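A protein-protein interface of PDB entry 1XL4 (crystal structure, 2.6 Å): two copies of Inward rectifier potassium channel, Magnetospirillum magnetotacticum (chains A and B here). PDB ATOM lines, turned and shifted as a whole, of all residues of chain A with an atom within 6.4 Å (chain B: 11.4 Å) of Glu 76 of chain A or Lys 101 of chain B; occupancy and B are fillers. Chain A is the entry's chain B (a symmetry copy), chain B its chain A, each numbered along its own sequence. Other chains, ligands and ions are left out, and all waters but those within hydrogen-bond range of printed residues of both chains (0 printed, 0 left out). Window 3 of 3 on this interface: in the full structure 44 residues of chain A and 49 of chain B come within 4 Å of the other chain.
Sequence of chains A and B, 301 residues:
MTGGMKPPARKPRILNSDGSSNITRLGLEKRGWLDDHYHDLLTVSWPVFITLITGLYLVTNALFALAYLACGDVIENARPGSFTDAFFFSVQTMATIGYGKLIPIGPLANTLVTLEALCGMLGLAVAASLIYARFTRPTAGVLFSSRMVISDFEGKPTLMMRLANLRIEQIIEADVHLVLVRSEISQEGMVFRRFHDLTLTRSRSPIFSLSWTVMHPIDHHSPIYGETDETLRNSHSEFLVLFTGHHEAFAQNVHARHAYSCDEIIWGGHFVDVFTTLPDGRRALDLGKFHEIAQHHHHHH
NZ of Lys 101 of chain B is in salt-bridge range of OE2 of Glu 76 of chain A, at 3.4 Å.
The backbone carbonyl oxygen (O) of Lys 101 of chain B sits close to the side-chain amide nitrogen (ND2) of Asn 77 of chain B (3.2 Å).
The backbone NH (N) of Ile 105 of chain A sits at hydrogen-bond distance from the backbone carbonyl oxygen (O) of Val 74 of chain A (2.7 Å).
The backbone NH (N) of Glu 76 of chain A is in hydrogen-bond range of the backbone carbonyl oxygen (O) of Ile 103 of chain A.
Among the printed residues, pairs that only touch across the chains: Gly 100 of chain A with Tyr 99 of chain B, Ile 103 of chain A with Tyr 99 of chain B, Ile 103 of chain A with Lys 101 of chain B, Pro 104 of chain A with Tyr 99 of chain B and Ile 105 of chain A with Lys 101 of chain B.
Ile 75 of chain A touches none of the printed residues of chain B.
Of chain B, only Lys 101 (3.4 Å) comes within 4 Å of Glu 76 of chain A.
Asn 77 of chain A touches none of the printed residues of chain B.
No residue of chain B comes within 4 Å of Ala 78 of chain A.
Of the printed residues of chain B, Gly 100 of chain A touches Tyr 99 (3.3 Å).
No residue of chain B comes within 4 Å of Leu 102 of chain A.
Pro 104 of chain A touches just one residue of chain B: Tyr 99.
Of chain B, only Lys 101 (3.8 Å) comes within 4 Å of Ile 105 of chain A.
Arg 79 of chain B touches none of the printed residues of chain A.
Of the printed residues of chain A, Tyr 99 of chain B touches Gly 100, Ile 103 and Pro 104.
Lys 101 of chain B touches three residues of chain A.
The nearest residue of chain A that does not touch Lys 101 of chain B is Pro 104 of chain A (4.1 Å).
The nearest printed residue of chain A that does not touch Tyr 99 of chain B is Leu 102 of chain A (5.3 Å).
Hydrophobic or aromatic side chains of chain B that line the printed part of chain A: Tyr 99.
Along chain B the printed residues that touch a printed residue of chain A span positions 99 to 101.
Hydrophobic or aromatic side chains of chain A within 4 Å of the printed part of chain B: Ile 103, Pro 104 and Ile 105.
Along chain A the printed residues that touch a printed residue of chain B span positions 76 to 105.
Among the printed residues, Asp or Glu carboxylates within 4 Å of a Lys or Arg side-chain nitrogen of the other chain: Glu 76 of chain A with Lys 101 of chain B (3.4 Å).
Glu 76 of chain A touches Lys 101 of chain B, but with the chains exchanged Lys 101 of chain A does not touch Glu 76 of chain B (14.2 Å).
Ile 103 of chain A touches Lys 101 of chain B, but with the chains exchanged Lys 101 of chain A does not touch Ile 103 of chain B (11.3 Å).
Ile 105 of chain A touches Lys 101 of chain B, but with the chains exchanged Lys 101 of chain A does not touch Ile 105 of chain B (18.1 Å).
Of the 6 pairs that touch across the chains among the printed residues, none has its exchanged pair printed and touching as well.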
ATOM      1  N   ASP A  73       4.616   8.203   7.617  1.00  0.00           N
ATOM      2  CA  ASP A  73       3.170   8.406   7.545  1.00  0.00           C
ATOM      3  C   ASP A  73       2.812   9.660   8.326  1.00  0.00           C
ATOM      4  O   ASP A  73       2.174   9.579   9.375  1.00  0.00           O
ATOM      5  CB  ASP A  73       2.420   7.205   8.141  1.00  0.00           C
ATOM      6  CG  ASP A  73       2.478   5.974   7.253  1.00  0.00           C
ATOM      7  OD1 ASP A  73       2.000   6.043   6.101  1.00  0.00           O
ATOM      8  OD2 ASP A  73       3.002   4.936   7.711  1.00  0.00           O
ATOM      9  N   VAL A  74       3.221  10.815   7.812  1.00  0.00           N
ATOM     10  CA  VAL A  74       2.951  12.076   8.486  1.00  0.00           C
ATOM     11  C   VAL A  74       1.689  12.794   7.999  1.00  0.00           C
ATOM     12  O   VAL A  74       1.424  13.931   8.390  1.00  0.00           O
ATOM     13  CB  VAL A  74       4.163  13.012   8.369  1.00  0.00           C
ATOM     14  CG1 VAL A  74       5.300  12.491   9.235  1.00  0.00           C
ATOM     15  CG2 VAL A  74       4.613  13.092   6.921  1.00  0.00           C
ATOM     16  N   ILE A  75       0.908  12.125   7.156  1.00  0.00           N
ATOM     17  CA  ILE A  75      -0.331  12.706   6.646  1.00  0.00           C
ATOM     18  C   ILE A  75      -1.514  11.885   7.143  1.00  0.00           C
ATOM     19  O   ILE A  75      -1.698  10.748   6.712  1.00  0.00           O
ATOM     20  CB  ILE A  75      -0.384  12.697   5.102  1.00  0.00           C
ATOM     21  CG1 ILE A  75       0.850  13.379   4.513  1.00  0.00           C
ATOM     22  CG2 ILE A  75      -1.641  13.409   4.630  1.00  0.00           C
ATOM     23  CD1 ILE A  75       0.945  13.259   3.008  1.00  0.00           C
ATOM     24  N   GLU A  76      -2.318  12.453   8.038  1.00  0.00           N
ATOM     25  CA  GLU A  76      -3.474  11.733   8.564  1.00  0.00           C
ATOM     26  C   GLU A  76      -4.467  11.314   7.482  1.00  0.00           C
ATOM     27  O   GLU A  76      -4.582  11.958   6.443  1.00  0.00           O
ATOM     28  CB  GLU A  76      -4.214  12.568   9.615  1.00  0.00           C
ATOM     29  CG  GLU A  76      -3.544  12.592  10.984  1.00  0.00           C
ATOM     30  CD  GLU A  76      -4.475  13.056  12.098  1.00  0.00           C
ATOM     31  OE1 GLU A  76      -5.449  12.333  12.399  1.00  0.00           O
ATOM     32  OE2 GLU A  76      -4.235  14.143  12.673  1.00  0.00           O
ATOM     33  N   ASN A  77      -5.177  10.222   7.748  1.00  0.00           N
ATOM     34  CA  ASN A  77      -6.185   9.692   6.840  1.00  0.00           C
ATOM     35  C   ASN A  77      -5.709   9.397   5.426  1.00  0.00           C
ATOM     36  O   ASN A  77      -6.512   9.382   4.491  1.00  0.00           O
ATOM     37  CB  ASN A  77      -7.380  10.643   6.794  1.00  0.00           C
ATOM     38  CG  ASN A  77      -8.108  10.713   8.115  1.00  0.00           C
ATOM     39  OD1 ASN A  77      -8.745   9.744   8.532  1.00  0.00           O
ATOM     40  ND2 ASN A  77      -8.009  11.852   8.790  1.00  0.00           N
ATOM     41  N   ALA A  78      -4.413   9.147   5.266  1.00  0.00           N
ATOM     42  CA  ALA A  78      -3.864   8.837   3.951  1.00  0.00           C
ATOM     43  C   ALA A  78      -3.261   7.435   3.918  1.00  0.00           C
ATOM     44  O   ALA A  78      -2.522   7.049   4.826  1.00  0.00           O
ATOM     45  CB  ALA A  78      -2.806   9.865   3.571  1.00  0.00           C
ATOM     46  N   GLY A 100      -9.063  19.341   4.639  1.00  0.00           N
ATOM     47  CA  GLY A 100      -9.067  19.070   6.056  1.00  0.00           C
ATOM     48  C   GLY A 100      -9.056  17.614   6.452  1.00  0.00           C
ATOM     49  O   GLY A 100      -8.890  17.317   7.627  1.00  0.00           O
ATOM     50  N   LYS A 101      -9.239  16.718   5.490  1.00  0.00           N
ATOM     51  CA  LYS A 101      -9.234  15.294   5.756  1.00  0.00           C
ATOM     52  C   LYS A 101      -7.781  14.822   5.783  1.00  0.00           C
ATOM     53  O   LYS A 101      -7.409  13.963   6.574  1.00  0.00           O
ATOM     54  CB  LYS A 101     -10.012  14.567   4.662  1.00  0.00           C
ATOM     55  CG  LYS A 101      -9.949  13.067   4.771  1.00  0.00           C
ATOM     56  CD  LYS A 101     -10.678  12.412   3.613  1.00  0.00           C
ATOM     57  CE  LYS A 101     -10.139  11.007   3.335  1.00  0.00           C
ATOM     58  NZ  LYS A 101     -10.775  10.392   2.127  1.00  0.00           N
ATOM     59  N   LEU A 102      -6.948  15.421   4.944  1.00  0.00           N
ATOM     60  CA  LEU A 102      -5.554  15.019   4.876  1.00  0.00           C
ATOM     61  C   LEU A 102      -4.537  15.807   5.699  1.00  0.00           C
ATOM     62  O   LEU A 102      -3.344  15.722   5.431  1.00  0.00           O
ATOM     63  CB  LEU A 102      -5.115  14.992   3.415  1.00  0.00           C
ATOM     64  CG  LEU A 102      -5.763  13.898   2.566  1.00  0.00           C
ATOM     65  CD1 LEU A 102      -5.465  14.116   1.100  1.00  0.00           C
ATOM     66  CD2 LEU A 102      -5.234  12.551   3.009  1.00  0.00           C
ATOM     67  N   ILE A 103      -4.985  16.543   6.709  1.00  0.00           N
ATOM     68  CA  ILE A 103      -4.074  17.334   7.549  1.00  0.00           C
ATOM     69  C   ILE A 103      -2.669  16.744   7.769  1.00  0.00           C
ATOM     70  O   ILE A 103      -2.444  15.552   7.583  1.00  0.00           O
ATOM     71  CB  ILE A 103      -4.683  17.588   8.937  1.00  0.00           C
ATOM     72  CG1 ILE A 103      -4.915  16.252   9.652  1.00  0.00           C
ATOM     73  CG2 ILE A 103      -5.977  18.376   8.796  1.00  0.00           C
ATOM     74  CD1 ILE A 103      -5.333  16.398  11.101  1.00  0.00           C
ATOM     75  N   PRO A 104      -1.705  17.589   8.178  1.00  0.00           N
ATOM     76  CA  PRO A 104      -0.316  17.187   8.434  1.00  0.00           C
ATOM     77  C   PRO A 104      -0.149  16.604   9.834  1.00  0.00           C
ATOM     78  O   PRO A 104      -1.041  16.731  10.674  1.00  0.00           O
ATOM     79  CB  PRO A 104       0.466  18.497   8.296  1.00  0.00           C
ATOM     80  CG  PRO A 104      -0.515  19.475   7.693  1.00  0.00           C
ATOM     81  CD  PRO A 104      -1.826  19.051   8.250  1.00  0.00           C
ATOM     82  N   ILE A 105       1.007  15.995  10.088  1.00  0.00           N
ATOM     83  CA  ILE A 105       1.292  15.394  11.386  1.00  0.00           C
ATOM     84  C   ILE A 105       2.759  15.498  11.793  1.00  0.00           C
ATOM     85  O   ILE A 105       3.641  15.014  11.086  1.00  0.00           O
ATOM     86  CB  ILE A 105       0.887  13.898  11.400  1.00  0.00           C
ATOM     87  CG1 ILE A 105      -0.635  13.778  11.382  1.00  0.00           C
ATOM     88  CG2 ILE A 105       1.444  13.201  12.639  1.00  0.00           C
ATOM     89  CD1 ILE A 105      -1.315  14.457  12.567  1.00  0.00           C
ATOM     90  N   VAL B  74      -6.386  30.339  22.412  1.00  0.00           N
ATOM     91  CA  VAL B  74      -7.505  30.602  21.516  1.00  0.00           C
ATOM     92  C   VAL B  74      -7.413  29.753  20.250  1.00  0.00           C
ATOM     93  O   VAL B  74      -8.215  29.903  19.328  1.00  0.00           O
ATOM     94  CB  VAL B  74      -7.566  32.096  21.139  1.00  0.00           C
ATOM     95  CG1 VAL B  74      -7.940  32.921  22.361  1.00  0.00           C
ATOM     96  CG2 VAL B  74      -6.219  32.550  20.602  1.00  0.00           C
ATOM     97  N   ILE B  75      -6.430  28.855  20.219  1.00  0.00           N
ATOM     98  CA  ILE B  75      -6.236  27.967  19.081  1.00  0.00           C
ATOM     99  C   ILE B  75      -6.810  26.601  19.443  1.00  0.00           C
ATOM    100  O   ILE B  75      -6.147  25.794  20.100  1.00  0.00           O
ATOM    101  CB  ILE B  75      -4.736  27.784  18.743  1.00  0.00           C
ATOM    102  CG1 ILE B  75      -3.994  29.117  18.867  1.00  0.00           C
ATOM    103  CG2 ILE B  75      -4.585  27.245  17.323  1.00  0.00           C
ATOM    104  CD1 ILE B  75      -4.477  30.184  17.918  1.00  0.00           C
ATOM    105  N   GLU B  76      -8.042  26.347  19.019  1.00  0.00           N
ATOM    106  CA  GLU B  76      -8.692  25.081  19.315  1.00  0.00           C
ATOM    107  C   GLU B  76      -7.915  23.896  18.745  1.00  0.00           C
ATOM    108  O   GLU B  76      -7.442  23.939  17.611  1.00  0.00           O
ATOM    109  CB  GLU B  76     -10.125  25.088  18.780  1.00  0.00           C
ATOM    110  CG  GLU B  76     -10.913  23.849  19.148  1.00  0.00           C
ATOM    111  CD  GLU B  76     -12.411  24.094  19.216  1.00  0.00           C
ATOM    112  OE1 GLU B  76     -13.015  24.472  18.188  1.00  0.00           O
ATOM    113  OE2 GLU B  76     -12.982  23.906  20.310  1.00  0.00           O
ATOM    114  N   ASN B  77      -7.791  22.844  19.552  1.00  0.00           N
ATOM    115  CA  ASN B  77      -7.073  21.622  19.190  1.00  0.00           C
ATOM    116  C   ASN B  77      -5.565  21.823  19.112  1.00  0.00           C
ATOM    117  O   ASN B  77      -4.858  21.035  18.490  1.00  0.00           O
ATOM    118  CB  ASN B  77      -7.594  21.055  17.865  1.00  0.00           C
ATOM    119  CG  ASN B  77      -8.936  20.365  18.014  1.00  0.00           C
ATOM    120  OD1 ASN B  77      -9.063  19.375  18.732  1.00  0.00           O
ATOM    121  ND2 ASN B  77      -9.948  20.887  17.335  1.00  0.00           N
ATOM    122  N   ALA B  78      -5.078  22.875  19.759  1.00  0.00           N
ATOM    123  CA  ALA B  78      -3.654  23.177  19.773  1.00  0.00           C
ATOM    124  C   ALA B  78      -3.092  23.024  21.184  1.00  0.00           C
ATOM    125  O   ALA B  78      -3.779  23.299  22.171  1.00  0.00           O
ATOM    126  CB  ALA B  78      -3.419  24.590  19.275  1.00  0.00           C
ATOM    127  N   ARG B  79      -1.838  22.590  21.277  1.00  0.00           N
ATOM    128  CA  ARG B  79      -1.191  22.406  22.570  1.00  0.00           C
ATOM    129  C   ARG B  79      -0.928  23.754  23.236  1.00  0.00           C
ATOM    130  O   ARG B  79      -0.240  24.608  22.681  1.00  0.00           O
ATOM    131  CB  ARG B  79       0.118  21.649  22.386  1.00  0.00           C
ATOM    132  CG  ARG B  79      -0.065  20.316  21.688  1.00  0.00           C
ATOM    133  CD  ARG B  79       1.272  19.706  21.337  1.00  0.00           C
ATOM    134  NE  ARG B  79       2.079  20.622  20.538  1.00  0.00           N
ATOM    135  CZ  ARG B  79       3.320  20.368  20.140  1.00  0.00           C
ATOM    136  NH1 ARG B  79       3.896  19.220  20.468  1.00  0.00           N
ATOM    137  NH2 ARG B  79       3.988  21.262  19.422  1.00  0.00           N
ATOM    138  N   THR B  84       5.103  26.191  18.337  1.00  0.00           N
ATOM    139  CA  THR B  84       5.013  25.333  17.168  1.00  0.00           C
ATOM    140  C   THR B  84       3.594  25.251  16.620  1.00  0.00           C
ATOM    141  O   THR B  84       3.365  25.479  15.435  1.00  0.00           O
ATOM    142  CB  THR B  84       5.496  23.916  17.518  1.00  0.00           C
ATOM    143  OG1 THR B  84       6.878  23.966  17.882  1.00  0.00           O
ATOM    144  CG2 THR B  84       5.314  22.970  16.339  1.00  0.00           C
ATOM    145  N   ASP B  85       2.648  24.919  17.490  1.00  0.00           N
ATOM    146  CA  ASP B  85       1.247  24.796  17.099  1.00  0.00           C
ATOM    147  C   ASP B  85       0.616  26.136  16.705  1.00  0.00           C
ATOM    148  O   ASP B  85      -0.221  26.192  15.802  1.00  0.00           O
ATOM    149  CB  ASP B  85       0.446  24.155  18.240  1.00  0.00           C
ATOM    150  CG  ASP B  85       0.777  22.679  18.432  1.00  0.00           C
ATOM    151  OD1 ASP B  85       1.965  22.313  18.299  1.00  0.00           O
ATOM    152  OD2 ASP B  85      -0.148  21.890  18.729  1.00  0.00           O
ATOM    153  N   ALA B  86       1.017  27.209  17.382  1.00  0.00           N
ATOM    154  CA  ALA B  86       0.478  28.530  17.084  1.00  0.00           C
ATOM    155  C   ALA B  86       1.107  29.065  15.801  1.00  0.00           C
ATOM    156  O   ALA B  86       0.462  29.785  15.035  1.00  0.00           O
ATOM    157  CB  ALA B  86       0.745  29.488  18.243  1.00  0.00           C
ATOM    158  N   PHE B  88       2.220  27.193  13.216  1.00  0.00           N
ATOM    159  CA  PHE B  88       1.646  26.480  12.087  1.00  0.00           C
ATOM    160  C   PHE B  88       0.177  26.844  11.900  1.00  0.00           C
ATOM    161  O   PHE B  88      -0.401  26.595  10.841  1.00  0.00           O
ATOM    162  CB  PHE B  88       1.829  24.976  12.274  1.00  0.00           C
ATOM    163  CG  PHE B  88       3.267  24.536  12.208  1.00  0.00           C
ATOM    164  CD1 PHE B  88       3.732  23.490  13.005  1.00  0.00           C
ATOM    165  CD2 PHE B  88       4.161  25.171  11.349  1.00  0.00           C
ATOM    166  CE1 PHE B  88       5.072  23.082  12.941  1.00  0.00           C
ATOM    167  CE2 PHE B  88       5.494  24.773  11.279  1.00  0.00           C
ATOM    168  CZ  PHE B  88       5.951  23.726  12.077  1.00  0.00           C
ATOM    169  N   PHE B  89      -0.429  27.433  12.927  1.00  0.00           N
ATOM    170  CA  PHE B  89      -1.814  27.866  12.803  1.00  0.00           C
ATOM    171  C   PHE B  89      -1.746  29.120  11.939  1.00  0.00           C
ATOM    172  O   PHE B  89      -2.491  29.269  10.966  1.00  0.00           O
ATOM    173  CB  PHE B  89      -2.422  28.233  14.159  1.00  0.00           C
ATOM    174  CG  PHE B  89      -3.793  28.851  14.052  1.00  0.00           C
ATOM    175  CD1 PHE B  89      -4.857  28.126  13.517  1.00  0.00           C
ATOM    176  CD2 PHE B  89      -4.009  30.174  14.436  1.00  0.00           C
ATOM    177  CE1 PHE B  89      -6.118  28.711  13.360  1.00  0.00           C
ATOM    178  CE2 PHE B  89      -5.268  30.768  14.282  1.00  0.00           C
ATOM    179  CZ  PHE B  89      -6.322  30.031  13.741  1.00  0.00           C
ATOM    180  N   SER B  90      -0.832  30.011  12.317  1.00  0.00           N
ATOM    181  CA  SER B  90      -0.603  31.265  11.619  1.00  0.00           C
ATOM    182  C   SER B  90      -0.409  30.972  10.137  1.00  0.00           C
ATOM    183  O   SER B  90      -1.178  31.448   9.305  1.00  0.00           O
ATOM    184  CB  SER B  90       0.639  31.949  12.196  1.00  0.00           C
ATOM    185  OG  SER B  90       0.741  33.298  11.769  1.00  0.00           O
ATOM    186  N   GLN B  92      -1.055  28.367   8.297  1.00  0.00           N
ATOM    187  CA  GLN B  92      -2.285  27.833   7.730  1.00  0.00           C
ATOM    188  C   GLN B  92      -3.317  28.905   7.456  1.00  0.00           C
ATOM    189  O   GLN B  92      -4.086  28.806   6.497  1.00  0.00           O
ATOM    190  CB  GLN B  92      -2.888  26.803   8.675  1.00  0.00           C
ATOM    191  CG  GLN B  92      -2.172  25.471   8.676  1.00  0.00           C
ATOM    192  CD  GLN B  92      -2.729  24.530   9.723  1.00  0.00           C
ATOM    193  OE1 GLN B  92      -3.948  24.431   9.898  1.00  0.00           O
ATOM    194  NE2 GLN B  92      -1.842  23.829  10.421  1.00  0.00           N
ATOM    195  N   THR B  93      -3.331  29.920   8.312  1.00  0.00           N
ATOM    196  CA  THR B  93      -4.267  31.031   8.201  1.00  0.00           C
ATOM    197  C   THR B  93      -3.805  32.033   7.143  1.00  0.00           C
ATOM    198  O   THR B  93      -4.532  32.341   6.193  1.00  0.00           O
ATOM    199  CB  THR B  93      -4.396  31.772   9.561  1.00  0.00           C
ATOM    200  OG1 THR B  93      -4.841  30.855  10.569  1.00  0.00           O
ATOM    201  CG2 THR B  93      -5.389  32.921   9.461  1.00  0.00           C
ATOM    202  N   ILE B  97      -4.653  28.192   3.856  1.00  0.00           N
ATOM    203  CA  ILE B  97      -4.826  26.760   3.626  1.00  0.00           C
ATOM    204  C   ILE B  97      -6.064  26.314   4.412  1.00  0.00           C
ATOM    205  O   ILE B  97      -6.947  25.625   3.883  1.00  0.00           O
ATOM    206  CB  ILE B  97      -3.594  25.962   4.098  1.00  0.00           C
ATOM    207  CG1 ILE B  97      -2.371  26.366   3.262  1.00  0.00           C
ATOM    208  CG2 ILE B  97      -3.869  24.467   3.990  1.00  0.00           C
ATOM    209  CD1 ILE B  97      -1.074  25.786   3.742  1.00  0.00           C
ATOM    210  N   GLY B  98      -6.113  26.741   5.673  1.00  0.00           N
ATOM    211  CA  GLY B  98      -7.239  26.444   6.544  1.00  0.00           C
ATOM    212  C   GLY B  98      -7.715  25.004   6.606  1.00  0.00           C
ATOM    213  O   GLY B  98      -8.855  24.698   6.246  1.00  0.00           O
ATOM    214  N   TYR B  99      -6.846  24.119   7.073  1.00  0.00           N
ATOM    215  CA  TYR B  99      -7.204  22.715   7.176  1.00  0.00           C
ATOM    216  C   TYR B  99      -8.521  22.515   7.937  1.00  0.00           C
ATOM    217  O   TYR B  99      -9.536  22.103   7.365  1.00  0.00           O
ATOM    218  CB  TYR B  99      -6.069  21.950   7.851  1.00  0.00           C
ATOM    219  CG  TYR B  99      -4.844  21.811   6.979  1.00  0.00           C
ATOM    220  CD1 TYR B  99      -3.614  22.334   7.376  1.00  0.00           C
ATOM    221  CD2 TYR B  99      -4.919  21.150   5.754  1.00  0.00           C
ATOM    222  CE1 TYR B  99      -2.480  22.198   6.565  1.00  0.00           C
ATOM    223  CE2 TYR B  99      -3.804  21.011   4.942  1.00  0.00           C
ATOM    224  CZ  TYR B  99      -2.590  21.532   5.353  1.00  0.00           C
ATOM    225  OH  TYR B  99      -1.476  21.366   4.563  1.00  0.00           O
ATOM    226  N   GLY B 100      -8.518  22.834   9.224  1.00  0.00           N
ATOM    227  CA  GLY B 100      -9.738  22.683   9.987  1.00  0.00           C
ATOM    228  C   GLY B 100      -9.531  22.146  11.385  1.00  0.00           C
ATOM    229  O   GLY B 100     -10.464  22.157  12.192  1.00  0.00           O
ATOM    230  N   LYS B 101      -8.329  21.665  11.680  1.00  0.00           N
ATOM    231  CA  LYS B 101      -8.046  21.144  12.999  1.00  0.00           C
ATOM    232  C   LYS B 101      -7.665  22.262  13.969  1.00  0.00           C
ATOM    233  O   LYS B 101      -8.160  22.305  15.094  1.00  0.00           O
ATOM    234  CB  LYS B 101      -6.914  20.106  12.934  1.00  0.00           C
ATOM    235  CG  LYS B 101      -6.502  19.583  14.308  1.00  0.00           C
ATOM    236  CD  LYS B 101      -5.722  18.267  14.262  1.00  0.00           C
ATOM    237  CE  LYS B 101      -4.321  18.413  13.668  1.00  0.00           C
ATOM    238  NZ  LYS B 101      -3.468  17.216  13.969  1.00  0.00           N
ATOM    239  N   LEU B 102      -6.822  23.191  13.530  1.00  0.00           N
ATOM    240  CA  LEU B 102      -6.366  24.262  14.412  1.00  0.00           C
ATOM    241  C   LEU B 102      -7.255  25.497  14.584  1.00  0.00           C
ATOM    242  O   LEU B 102      -6.877  26.427  15.297  1.00  0.00           O
ATOM    243  CB  LEU B 102      -4.973  24.712  13.985  1.00  0.00           C
ATOM    244  CG  LEU B 102      -3.840  23.686  14.003  1.00  0.00           C
ATOM    245  CD1 LEU B 102      -2.566  24.342  13.515  1.00  0.00           C
ATOM    246  CD2 LEU B 102      -3.644  23.151  15.398  1.00  0.00           C
ATOM    247  N   ILE B 103      -8.427  25.508  13.957  1.00  0.00           N
ATOM    248  CA  ILE B 103      -9.373  26.638  14.035  1.00  0.00           C
ATOM    249  C   ILE B 103      -9.277  27.582  15.256  1.00  0.00           C
ATOM    250  O   ILE B 103      -8.968  27.158  16.370  1.00  0.00           O
ATOM    251  CB  ILE B 103     -10.817  26.131  13.979  1.00  0.00           C
ATOM    252  CG1 ILE B 103     -11.165  25.435  15.297  1.00  0.00           C
ATOM    253  CG2 ILE B 103     -10.976  25.155  12.824  1.00  0.00           C
ATOM    254  CD1 ILE B 103     -12.621  25.093  15.433  1.00  0.00           C
ATOM    255  N   PRO B 104      -9.577  28.878  15.054  1.00  0.00           N
ATOM    256  CA  PRO B 104      -9.542  29.925  16.088  1.00  0.00           C
ATOM    257  C   PRO B 104     -10.547  29.676  17.211  1.00  0.00           C
ATOM    258  O   PRO B 104     -11.280  28.691  17.178  1.00  0.00           O
ATOM    259  CB  PRO B 104      -9.895  31.196  15.316  1.00  0.00           C
ATOM    260  CG  PRO B 104      -9.552  30.867  13.906  1.00  0.00           C
ATOM    261  CD  PRO B 104     -10.002  29.448  13.767  1.00  0.00           C
ATOM    262  N   ILE B 105     -10.584  30.583  18.189  1.00  0.00           N
ATOM    263  CA  ILE B 105     -11.501  30.485  19.329  1.00  0.00           C
ATOM    264  C   ILE B 105     -11.741  31.848  19.987  1.00  0.00           C
ATOM    265  O   ILE B 105     -10.825  32.438  20.556  1.00  0.00           O
ATOM    266  CB  ILE B 105     -10.961  29.524  20.427  1.00  0.00           C
ATOM    267  CG1 ILE B 105     -10.970  28.075  19.929  1.00  0.00           C
ATOM    268  CG2 ILE B 105     -11.811  29.643  21.687  1.00  0.00           C
ATOM    269  CD1 ILE B 105     -12.359  27.523  19.628  1.00  0.00           C
